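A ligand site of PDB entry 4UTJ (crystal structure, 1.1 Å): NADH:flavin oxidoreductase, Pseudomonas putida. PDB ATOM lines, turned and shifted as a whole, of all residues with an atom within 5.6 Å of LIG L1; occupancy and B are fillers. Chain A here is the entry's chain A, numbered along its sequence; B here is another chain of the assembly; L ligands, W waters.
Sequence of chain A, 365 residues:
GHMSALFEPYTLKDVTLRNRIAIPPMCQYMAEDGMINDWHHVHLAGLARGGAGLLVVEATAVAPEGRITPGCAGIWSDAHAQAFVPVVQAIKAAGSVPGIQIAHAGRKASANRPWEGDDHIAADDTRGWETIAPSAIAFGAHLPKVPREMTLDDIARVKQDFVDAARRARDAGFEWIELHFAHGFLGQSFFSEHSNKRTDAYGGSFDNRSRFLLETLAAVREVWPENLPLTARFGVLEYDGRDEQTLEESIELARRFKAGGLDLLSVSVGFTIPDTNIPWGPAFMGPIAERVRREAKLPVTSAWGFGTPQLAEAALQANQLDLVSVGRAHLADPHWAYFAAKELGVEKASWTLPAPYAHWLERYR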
ATOM      1  N   PRO A  24      10.992  10.704  -2.154  1.00  0.00           N
ATOM      2  CA  PRO A  24      11.260  11.847  -1.292  1.00  0.00           C
ATOM      3  C   PRO A  24       9.953  12.342  -0.702  1.00  0.00           C
ATOM      4  O   PRO A  24       8.852  12.008  -1.189  1.00  0.00           O
ATOM      5  CB  PRO A  24      11.824  12.878  -2.280  1.00  0.00           C
ATOM      6  CG  PRO A  24      11.085  12.577  -3.559  1.00  0.00           C
ATOM      7  CD  PRO A  24      10.960  11.091  -3.589  1.00  0.00           C
ATOM      8  N   PRO A  25      10.053  13.152   0.353  1.00  0.00           N
ATOM      9  CA  PRO A  25       8.856  13.726   0.965  1.00  0.00           C
ATOM     10  C   PRO A  25       8.047  14.504  -0.064  1.00  0.00           C
ATOM     11  O   PRO A  25       8.575  15.325  -0.802  1.00  0.00           O
ATOM     12  CB  PRO A  25       9.426  14.636   2.070  1.00  0.00           C
ATOM     13  CG  PRO A  25      10.843  14.937   1.619  1.00  0.00           C
ATOM     14  CD  PRO A  25      11.292  13.652   0.970  1.00  0.00           C
ATOM     15  N   MET A  26       6.731  14.255  -0.079  1.00  0.00           N
ATOM     16  CA  MET A  26       5.807  14.968  -0.956  1.00  0.00           C
ATOM     17  C   MET A  26       4.525  15.282  -0.196  1.00  0.00           C
ATOM     18  O   MET A  26       3.633  14.442  -0.034  1.00  0.00           O
ATOM     19  CB  MET A  26       5.484  14.165  -2.228  1.00  0.00           C
ATOM     20  CG  MET A  26       6.653  14.111  -3.201  1.00  0.00           C
ATOM     21  SD  MET A  26       6.259  13.276  -4.747  1.00  0.00           S
ATOM     22  CE  MET A  26       6.247  11.603  -4.132  1.00  0.00           C
ATOM     23  N   CYS A  27       4.418  16.522   0.205  1.00  0.00           N
ATOM     24  CA  CYS A  27       3.207  17.037   0.827  1.00  0.00           C
ATOM     25  C   CYS A  27       1.958  16.690   0.033  1.00  0.00           C
ATOM     26  O   CYS A  27       1.909  16.838  -1.212  1.00  0.00           O
ATOM     27  CB  CYS A  27       3.294  18.541   0.996  1.00  0.00           C
ATOM     28  SG  CYS A  27       4.272  19.102   2.379  1.00  0.00           S
ATOM     29  N   GLN A  28       0.921  16.278   0.771  1.00  0.00           N
ATOM     30  CA  GLN A  28      -0.362  15.908   0.223  1.00  0.00           C
ATOM     31  C   GLN A  28      -1.467  16.922   0.498  1.00  0.00           C
ATOM     32  O   GLN A  28      -2.511  16.879  -0.158  1.00  0.00           O
ATOM     33  CB  GLN A  28      -0.740  14.534   0.770  1.00  0.00           C
ATOM     34  CG  GLN A  28       0.222  13.438   0.372  1.00  0.00           C
ATOM     35  CD  GLN A  28       0.230  13.208  -1.111  1.00  0.00           C
ATOM     36  OE1 GLN A  28      -0.724  12.679  -1.671  1.00  0.00           O
ATOM     37  NE2 GLN A  28       1.313  13.636  -1.761  1.00  0.00           N
ATOM     38  N   TYR A  29      -1.280  17.775   1.507  1.00  0.00           N
ATOM     39  CA  TYR A  29      -2.233  18.814   1.839  1.00  0.00           C
ATOM     40  C   TYR A  29      -3.615  18.281   2.208  1.00  0.00           C
ATOM     41  O   TYR A  29      -4.620  18.955   1.993  1.00  0.00           O
ATOM     42  CB  TYR A  29      -2.318  19.893   0.736  1.00  0.00           C
ATOM     43  CG  TYR A  29      -0.969  20.358   0.248  1.00  0.00           C
ATOM     44  CD1 TYR A  29      -0.323  21.418   0.873  1.00  0.00           C
ATOM     45  CD2 TYR A  29      -0.319  19.727  -0.793  1.00  0.00           C
ATOM     46  CE1 TYR A  29       0.940  21.843   0.454  1.00  0.00           C
ATOM     47  CE2 TYR A  29       0.944  20.142  -1.202  1.00  0.00           C
ATOM     48  CZ  TYR A  29       1.548  21.205  -0.595  1.00  0.00           C
ATOM     49  OH  TYR A  29       2.777  21.593  -1.032  1.00  0.00           O
ATOM     50  N   GLU A  58       6.041  13.017   3.813  1.00  0.00           N
ATOM     51  CA  GLU A  58       5.976  14.445   3.592  1.00  0.00           C
ATOM     52  C   GLU A  58       6.390  15.288   4.787  1.00  0.00           C
ATOM     53  O   GLU A  58       6.241  14.878   5.944  1.00  0.00           O
ATOM     54  CB  GLU A  58       4.534  14.840   3.227  1.00  0.00           C
ATOM     55  CG  GLU A  58       3.507  14.564   4.343  1.00  0.00           C
ATOM     56  CD  GLU A  58       2.094  14.583   3.772  1.00  0.00           C
ATOM     57  OE1 GLU A  58       1.513  15.688   3.637  1.00  0.00           O
ATOM     58  OE2 GLU A  58       1.586  13.506   3.402  1.00  0.00           O
ATOM     59  N   ALA A  59       6.800  16.536   4.494  1.00  0.00           N
ATOM     60  CA  ALA A  59       7.090  17.541   5.518  1.00  0.00           C
ATOM     61  C   ALA A  59       5.997  17.516   6.582  1.00  0.00           C
ATOM     62  O   ALA A  59       4.836  17.850   6.313  1.00  0.00           O
ATOM     63  CB  ALA A  59       7.173  18.906   4.896  1.00  0.00           C
ATOM     64  N   GLN A 101      10.099  13.248   7.112  1.00  0.00           N
ATOM     65  CA  GLN A 101      10.724  14.567   7.106  1.00  0.00           C
ATOM     66  C   GLN A 101      10.009  15.441   8.128  1.00  0.00           C
ATOM     67  O   GLN A 101       8.805  15.653   8.016  1.00  0.00           O
ATOM     68  CB  GLN A 101      10.640  15.186   5.711  1.00  0.00           C
ATOM     69  CG  GLN A 101      11.414  16.461   5.634  1.00  0.00           C
ATOM     70  CD  GLN A 101      11.160  17.215   4.341  1.00  0.00           C
ATOM     71  OE1 GLN A 101      10.021  17.580   4.074  1.00  0.00           O
ATOM     72  NE2 GLN A 101      12.203  17.452   3.558  1.00  0.00           N
ATOM     73  N   GLU A 178      14.526  12.778   8.443  1.00  0.00           N
ATOM     74  CA  GLU A 178      15.099  13.849   7.626  1.00  0.00           C
ATOM     75  C   GLU A 178      14.687  15.178   8.229  1.00  0.00           C
ATOM     76  O   GLU A 178      13.498  15.491   8.318  1.00  0.00           O
ATOM     77  CB  GLU A 178      14.634  13.743   6.188  1.00  0.00           C
ATOM     78  CG  GLU A 178      15.322  14.766   5.275  1.00  0.00           C
ATOM     79  CD  GLU A 178      14.851  14.625   3.832  1.00  0.00           C
ATOM     80  OE1 GLU A 178      15.146  13.612   3.171  1.00  0.00           O
ATOM     81  OE2 GLU A 178      14.151  15.507   3.330  1.00  0.00           O
ATOM     82  N   HIS A 180      14.153  18.994   7.749  1.00  0.00           N
ATOM     83  CA  HIS A 180      13.904  19.837   6.587  1.00  0.00           C
ATOM     84  C   HIS A 180      14.550  21.202   6.746  1.00  0.00           C
ATOM     85  O   HIS A 180      13.935  22.155   7.229  1.00  0.00           O
ATOM     86  CB  HIS A 180      12.419  19.997   6.337  1.00  0.00           C
ATOM     87  CG  HIS A 180      12.127  20.512   4.974  1.00  0.00           C
ATOM     88  ND1 HIS A 180      13.115  20.969   4.120  1.00  0.00           N
ATOM     89  CD2 HIS A 180      10.955  20.565   4.292  1.00  0.00           C
ATOM     90  CE1 HIS A 180      12.545  21.248   2.966  1.00  0.00           C
ATOM     91  NE2 HIS A 180      11.238  21.000   3.031  1.00  0.00           N
ATOM     92  N   HIS A 183      14.641  24.660   1.113  1.00  0.00           N
ATOM     93  CA  HIS A 183      13.448  25.160   0.428  1.00  0.00           C
ATOM     94  C   HIS A 183      12.883  26.427   1.036  1.00  0.00           C
ATOM     95  O   HIS A 183      11.715  26.756   0.862  1.00  0.00           O
ATOM     96  CB  HIS A 183      12.402  24.044   0.269  1.00  0.00           C
ATOM     97  CG  HIS A 183      12.919  22.873  -0.505  1.00  0.00           C
ATOM     98  ND1 HIS A 183      12.236  21.675  -0.568  1.00  0.00           N
ATOM     99  CD2 HIS A 183      14.046  22.692  -1.244  1.00  0.00           C
ATOM    100  CE1 HIS A 183      12.915  20.823  -1.309  1.00  0.00           C
ATOM    101  NE2 HIS A 183      14.024  21.412  -1.738  1.00  0.00           N
ATOM    102  N   ARG A 233      17.704  17.544   4.684  1.00  0.00           N
ATOM    103  CA  ARG A 233      17.625  18.150   3.367  1.00  0.00           C
ATOM    104  C   ARG A 233      18.101  19.585   3.513  1.00  0.00           C
ATOM    105  O   ARG A 233      17.729  20.279   4.462  1.00  0.00           O
ATOM    106  CB  ARG A 233      16.193  18.097   2.804  1.00  0.00           C
ATOM    107  CG  ARG A 233      16.158  18.311   1.264  1.00  0.00           C
ATOM    108  CD  ARG A 233      14.825  17.935   0.651  1.00  0.00           C
ATOM    109  NE  ARG A 233      15.023  17.489  -0.725  1.00  0.00           N
ATOM    110  CZ  ARG A 233      14.058  17.072  -1.543  1.00  0.00           C
ATOM    111  NH1 ARG A 233      12.795  17.140  -1.190  1.00  0.00           N
ATOM    112  NH2 ARG A 233      14.411  16.536  -2.705  1.00  0.00           N
ATOM    113  N   ALA A 303      17.182  15.067  -6.276  1.00  0.00           N
ATOM    114  CA  ALA A 303      15.924  14.888  -6.982  1.00  0.00           C
ATOM    115  C   ALA A 303      15.854  15.940  -8.092  1.00  0.00           C
ATOM    116  O   ALA A 303      16.626  16.895  -8.110  1.00  0.00           O
ATOM    117  CB  ALA A 303      14.763  15.064  -6.018  1.00  0.00           C
ATOM    118  N   TRP A 304      14.866  15.717  -8.947  1.00  0.00           N
ATOM    119  CA  TRP A 304      14.357  16.570 -10.025  1.00  0.00           C
ATOM    120  C   TRP A 304      14.692  15.924 -11.347  1.00  0.00           C
ATOM    121  O   TRP A 304      15.812  16.022 -11.857  1.00  0.00           O
ATOM    122  CB  TRP A 304      14.791  18.019 -10.005  1.00  0.00           C
ATOM    123  CG  TRP A 304      14.038  18.770 -11.100  1.00  0.00           C
ATOM    124  CD1 TRP A 304      14.304  18.775 -12.471  1.00  0.00           C
ATOM    125  CD2 TRP A 304      12.879  19.580 -10.921  1.00  0.00           C
ATOM    126  NE1 TRP A 304      13.386  19.544 -13.111  1.00  0.00           N
ATOM    127  CE2 TRP A 304      12.501  20.045 -12.205  1.00  0.00           C
ATOM    128  CE3 TRP A 304      12.132  19.961  -9.813  1.00  0.00           C
ATOM    129  CZ2 TRP A 304      11.399  20.877 -12.394  1.00  0.00           C
ATOM    130  CZ3 TRP A 304      11.038  20.785 -10.010  1.00  0.00           C
ATOM    131  CH2 TRP A 304      10.688  21.240 -11.294  1.00  0.00           C
ATOM    132  N   GLY A 305      13.697  15.228 -11.885  1.00  0.00           N
ATOM    133  CA  GLY A 305      13.832  14.590 -13.173  1.00  0.00           C
ATOM    134  C   GLY A 305      14.500  13.232 -13.230  1.00  0.00           C
ATOM    135  O   GLY A 305      14.846  12.806 -14.331  1.00  0.00           O
ATOM    136  N   PHE A 306      14.676  12.539 -12.108  1.00  0.00           N
ATOM    137  CA  PHE A 306      15.218  11.186 -12.132  1.00  0.00           C
ATOM    138  C   PHE A 306      14.203  10.060 -12.421  1.00  0.00           C
ATOM    139  O   PHE A 306      14.584   8.896 -12.389  1.00  0.00           O
ATOM    140  CB  PHE A 306      15.995  10.908 -10.833  1.00  0.00           C
ATOM    141  CG  PHE A 306      17.254  11.708 -10.696  1.00  0.00           C
ATOM    142  CD1 PHE A 306      18.392  11.342 -11.381  1.00  0.00           C
ATOM    143  CD2 PHE A 306      17.312  12.817  -9.863  1.00  0.00           C
ATOM    144  CE1 PHE A 306      19.546  12.068 -11.230  1.00  0.00           C
ATOM    145  CE2 PHE A 306      18.470  13.546  -9.699  1.00  0.00           C
ATOM    146  CZ  PHE A 306      19.604  13.167 -10.387  1.00  0.00           C
ATOM    147  N   GLY A 307      12.960  10.399 -12.747  1.00  0.00           N
ATOM    148  CA  GLY A 307      11.984   9.399 -13.139  1.00  0.00           C
ATOM    149  C   GLY A 307      12.216   8.751 -14.495  1.00  0.00           C
ATOM    150  O   GLY A 307      11.486   7.851 -14.892  1.00  0.00           O
ATOM    151  N   SER A 325      16.257   9.984  -5.645  1.00  0.00           N
ATOM    152  CA  SER A 325      14.912  10.353  -5.181  1.00  0.00           C
ATOM    153  C   SER A 325      14.037  10.619  -6.415  1.00  0.00           C
ATOM    154  O   SER A 325      14.400  11.415  -7.282  1.00  0.00           O
ATOM    155  CB  SER A 325      14.979  11.570  -4.269  1.00  0.00           C
ATOM    156  OG  SER A 325      15.658  11.233  -3.061  1.00  0.00           O
ATOM    157  N   VAL A 326      12.890   9.939  -6.449  1.00  0.00           N
ATOM    158  CA  VAL A 326      11.948   9.981  -7.578  1.00  0.00           C
ATOM    159  C   VAL A 326      10.579  10.337  -7.027  1.00  0.00           C
ATOM    160  O   VAL A 326       9.932   9.539  -6.339  1.00  0.00           O
ATOM    161  CB  VAL A 326      11.937   8.629  -8.303  1.00  0.00           C
ATOM    162  CG1 VAL A 326      10.905   8.676  -9.449  1.00  0.00           C
ATOM    163  CG2 VAL A 326      13.305   8.255  -8.811  1.00  0.00           C
ATOM    164  N   GLY A 327      10.143  11.555  -7.297  1.00  0.00           N
ATOM    165  CA  GLY A 327       8.937  12.122  -6.712  1.00  0.00           C
ATOM    166  C   GLY A 327       7.713  12.047  -7.613  1.00  0.00           C
ATOM    167  O   GLY A 327       6.879  11.142  -7.487  1.00  0.00           O
ATOM    168  N   ARG A 328       7.585  13.006  -8.538  1.00  0.00           N
ATOM    169  CA  ARG A 328       6.371  13.084  -9.355  1.00  0.00           C
ATOM    170  C   ARG A 328       6.084  11.830 -10.148  1.00  0.00           C
ATOM    171  O   ARG A 328       4.910  11.495 -10.328  1.00  0.00           O
ATOM    172  CB  ARG A 328       6.438  14.320 -10.247  1.00  0.00           C
ATOM    173  CG  ARG A 328       6.137  15.612  -9.489  1.00  0.00           C
ATOM    174  CD  ARG A 328       6.467  16.860 -10.243  1.00  0.00           C
ATOM    175  NE  ARG A 328       7.907  16.979 -10.415  1.00  0.00           N
ATOM    176  CZ  ARG A 328       8.486  17.946 -11.096  1.00  0.00           C
ATOM    177  NH1 ARG A 328       7.746  18.882 -11.665  1.00  0.00           N
ATOM    178  NH2 ARG A 328       9.803  17.942 -11.244  1.00  0.00           N
ATOM    179  N   ALA A 329       7.107  11.102 -10.597  1.00  0.00           N
ATOM    180  CA  ALA A 329       6.826   9.878 -11.330  1.00  0.00           C
ATOM    181  C   ALA A 329       6.056   8.882 -10.472  1.00  0.00           C
ATOM    182  O   ALA A 329       5.337   8.048 -11.033  1.00  0.00           O
ATOM    183  CB  ALA A 329       8.080   9.259 -11.866  1.00  0.00           C
ATOM    184  N   LEU A 331       3.772   9.818  -8.146  1.00  0.00           N
ATOM    185  CA  LEU A 331       2.387  10.301  -8.161  1.00  0.00           C
ATOM    186  C   LEU A 331       1.679   9.820  -9.409  1.00  0.00           C
ATOM    187  O   LEU A 331       0.521   9.381  -9.372  1.00  0.00           O
ATOM    188  CB  LEU A 331       2.334  11.818  -8.063  1.00  0.00           C
ATOM    189  CG  LEU A 331       3.084  12.471  -6.891  1.00  0.00           C
ATOM    190  CD1 LEU A 331       2.907  13.981  -6.902  1.00  0.00           C
ATOM    191  CD2 LEU A 331       2.687  11.879  -5.540  1.00  0.00           C
ATOM    192  N   PRO B 356      -4.253  16.119  -5.033  1.00  0.00           N
ATOM    193  CA  PRO B 356      -2.872  16.047  -4.546  1.00  0.00           C
ATOM    194  C   PRO B 356      -1.882  15.419  -5.527  1.00  0.00           C
ATOM    195  O   PRO B 356      -0.682  15.550  -5.331  1.00  0.00           O
ATOM    196  CB  PRO B 356      -2.992  15.214  -3.271  1.00  0.00           C
ATOM    197  CG  PRO B 356      -4.415  15.364  -2.838  1.00  0.00           C
ATOM    198  CD  PRO B 356      -5.187  15.429  -4.121  1.00  0.00           C
ATOM    199  N   TRP B 360       0.117  18.583  -9.655  1.00  0.00           N
ATOM    200  CA  TRP B 360       1.554  18.541  -9.918  1.00  0.00           C
ATOM    201  C   TRP B 360       1.892  17.876 -11.229  1.00  0.00           C
ATOM    202  O   TRP B 360       3.009  18.008 -11.716  1.00  0.00           O
ATOM    203  CB  TRP B 360       2.250  17.780  -8.795  1.00  0.00           C
ATOM    204  CG  TRP B 360       1.966  18.360  -7.467  1.00  0.00           C
ATOM    205  CD1 TRP B 360       1.045  17.925  -6.549  1.00  0.00           C
ATOM    206  CD2 TRP B 360       2.569  19.515  -6.918  1.00  0.00           C
ATOM    207  NE1 TRP B 360       1.064  18.749  -5.463  1.00  0.00           N
ATOM    208  CE2 TRP B 360       2.014  19.718  -5.643  1.00  0.00           C
ATOM    209  CE3 TRP B 360       3.561  20.380  -7.362  1.00  0.00           C
ATOM    210  CZ2 TRP B 360       2.409  20.768  -4.832  1.00  0.00           C
ATOM    211  CZ3 TRP B 360       3.959  21.408  -6.563  1.00  0.00           C
ATOM    212  CH2 TRP B 360       3.391  21.595  -5.295  1.00  0.00           C
HETATM  213  N1  LIG L   1      10.166  18.480  -0.841  1.00  0.00           N
HETATM  214  C1  LIG L   1      10.407  18.440   0.476  1.00  0.00           C
HETATM  215  O1  LIG L   1      11.577  18.517   0.938  1.00  0.00           O
HETATM  216  N2  LIG L   1       9.343  18.247   1.363  1.00  0.00           N
HETATM  217  C2  LIG L   1       8.081  18.042   0.992  1.00  0.00           C
HETATM  218  O2  LIG L   1       7.199  17.721   1.795  1.00  0.00           O
HETATM  219  C3  LIG L   1       7.818  18.238  -0.429  1.00  0.00           C
HETATM  220  N3  LIG L   1       6.532  18.200  -0.884  1.00  0.00           N
HETATM  221  C4  LIG L   1       6.341  18.095  -2.246  1.00  0.00           C
HETATM  222  C5  LIG L   1       5.034  17.808  -2.720  1.00  0.00           C
HETATM  223  C6  LIG L   1       4.807  17.473  -4.063  1.00  0.00           C
HETATM  224  C7  LIG L   1       3.490  16.974  -4.440  1.00  0.00           C
HETATM  225  C8  LIG L   1       5.884  17.549  -4.966  1.00  0.00           C
HETATM  226  C9  LIG L   1       5.685  17.240  -6.392  1.00  0.00           C
HETATM  227  C10 LIG L   1       7.150  17.960  -4.498  1.00  0.00           C
HETATM  228  C11 LIG L   1       7.416  18.097  -3.123  1.00  0.00           C
HETATM  229  N4  LIG L   1       8.712  18.294  -2.639  1.00  0.00           N
HETATM  230  C12 LIG L   1       8.905  18.367  -1.279  1.00  0.00           C
HETATM  231  C13 LIG L   1       9.858  18.146  -3.575  1.00  0.00           C
HETATM  232  C14 LIG L   1      10.088  16.678  -3.942  1.00  0.00           C
HETATM  233  O3  LIG L   1      10.574  15.950  -2.809  1.00  0.00           O
HETATM  234  C15 LIG L   1      11.125  16.513  -5.059  1.00  0.00           C
HETATM  235  O4  LIG L   1      12.387  17.036  -4.638  1.00  0.00           O
HETATM  236  C16 LIG L   1      10.722  17.204  -6.356  1.00  0.00           C
HETATM  237  O5  LIG L   1       9.371  16.911  -6.708  1.00  0.00           O
HETATM  238  C17 LIG L   1      11.650  16.869  -7.535  1.00  0.00           C
HETATM  239  O6  LIG L   1      11.679  15.475  -7.851  1.00  0.00           O
HETATM  240  P1  LIG L   1      10.797  14.913  -9.084  1.00  0.00           P
HETATM  241  O7  LIG L   1       9.344  15.183  -8.752  1.00  0.00           O
HETATM  242  O8  LIG L   1      11.221  15.646 -10.323  1.00  0.00           O
HETATM  243  O9  LIG L   1      11.143  13.461  -9.081  1.00  0.00           O
HETATM  244  C1  LG2 L   2       6.166  21.393  -1.225  1.00  0.00           C
HETATM  245  C2  LG2 L   2       6.269  21.359   0.076  1.00  0.00           C
HETATM  246  C3  LG2 L   2       7.492  21.366   0.719  1.00  0.00           C
HETATM  247  C4  LG2 L   2       8.706  21.441   0.007  1.00  0.00           C
HETATM  248  C5  LG2 L   2       8.642  21.480  -1.407  1.00  0.00           C
HETATM  249  C6  LG2 L   2       7.300  21.446  -2.050  1.00  0.00           C
HETATM  250  C7  LG2 L   2       7.278  21.482  -3.446  1.00  0.00           C
HETATM  251  C8  LG2 L   2       8.409  21.516  -4.121  1.00  0.00           C
HETATM  252  C9  LG2 L   2       9.656  21.540  -3.521  1.00  0.00           C
HETATM  253  O1  LG2 L   2       9.699  21.520  -2.158  1.00  0.00           O
HETATM  254  O2  LG2 L   2      10.720  21.578  -4.083  1.00  0.00           O
HETATM  255  O3  LG2 L   2       9.834  21.428   0.618  1.00  0.00           O
HETATM  256  O   HOH W   1       9.812  11.829 -10.865  1.00  0.00           O
HETATM  257  O   HOH W   2      10.198  14.938 -12.757  1.00  0.00           O
HETATM  258  O   HOH W   3       8.750  19.676  -7.613  1.00  0.00           O
HETATM  259  O   HOH W   4      13.794  13.082  -9.337  1.00  0.00           O
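The backbone NH of Cys 27 sits at hydrogen-bond distance from a nitrogen (N3) of LIG L1 (2.9 Å). An oxygen (O3) of LG2 L2 is in hydrogen-bond range of a ring nitrogen (ND1) of His 183. N of Gly 327 is in hydrogen-bond range of O9 of LIG L1. NE2 of His 180 lies within hydrogen-bond range of O1 of LIG L1, 3.3 Å away. The side-chain sulfur of Cys 27 is in hydrogen-bond range of an oxygen (O2) of LIG L1 (3.3 Å). O of Pro 25 lies within hydrogen-bond range of O3 of LIG L1, 2.9 Å away. N of Ala 59 lies within hydrogen-bond range of O2 of LIG L1, at 3.0 Å. O1 of LIG L1 is in hydrogen-bond range of NH1 of Arg 233 (2.8 Å). The backbone NH (N) of Gly 305 sits at hydrogen-bond distance from an oxygen (O8) of LIG L1, 3.0 Å away. A ring nitrogen (NE2) of His 180 sits at hydrogen-bond distance from an oxygen (O3) of LG2 L2. OE1 of Gln 101 is in hydrogen-bond range of N2 of LIG L1 (2.9 Å). The backbone NH (N) of Arg 328 sits at hydrogen-bond distance from an oxygen (O7) of LIG L1 (2.8 Å). The guanidinium group of Arg 328 is in salt-bridge range of an oxygen (O7) of LIG L1. An oxygen (O6) of LIG L1 sits at hydrogen-bond distance from the backbone NH of Trp 304, 3.4 Å away.
A nitrogen (N2) of LIG L1 lies close to an oxygen (O3) of LG2 L2, at 3.3 Å.
The side-chain carboxylate of Glu 58 is in hydrogen-bond range of the backbone NH of Gln 28. The side-chain amide oxygen of Gln 101 sits close to the backbone NH of Ala 59, at 3.4 Å. The side-chain carboxylate of Glu 178 is in hydrogen-bond range of the side-chain amide nitrogen of Gln 101 (2.8 Å). NE2 of Gln 28 is in hydrogen-bond range of O of Met 26 (3.0 Å).
Residues that only touch LIG L1: Trp 360 of chain B (3.2 Å), Met 26 (3.3 Å), Pro 24 (3.4 Å), Ala 303 (3.4 Å), His 183 (3.5 Å), Val 326 (3.8 Å), Leu 331 (3.9 Å) and Glu 58 (3.9 Å). The nearest printed residue that does not touch LIG L1 is Ser 325 (4.2 Å).
Water W2 lies within hydrogen-bond range of an oxygen (O8) of LIG L1 (2.7 Å) and the guanidinium group of Arg 328 (3.4 Å). Water W1 lies within hydrogen-bond range of O9 of LIG L1 (2.8 Å), N of Ala 329 (2.8 Å) and N of Arg 328 (3.4 Å).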
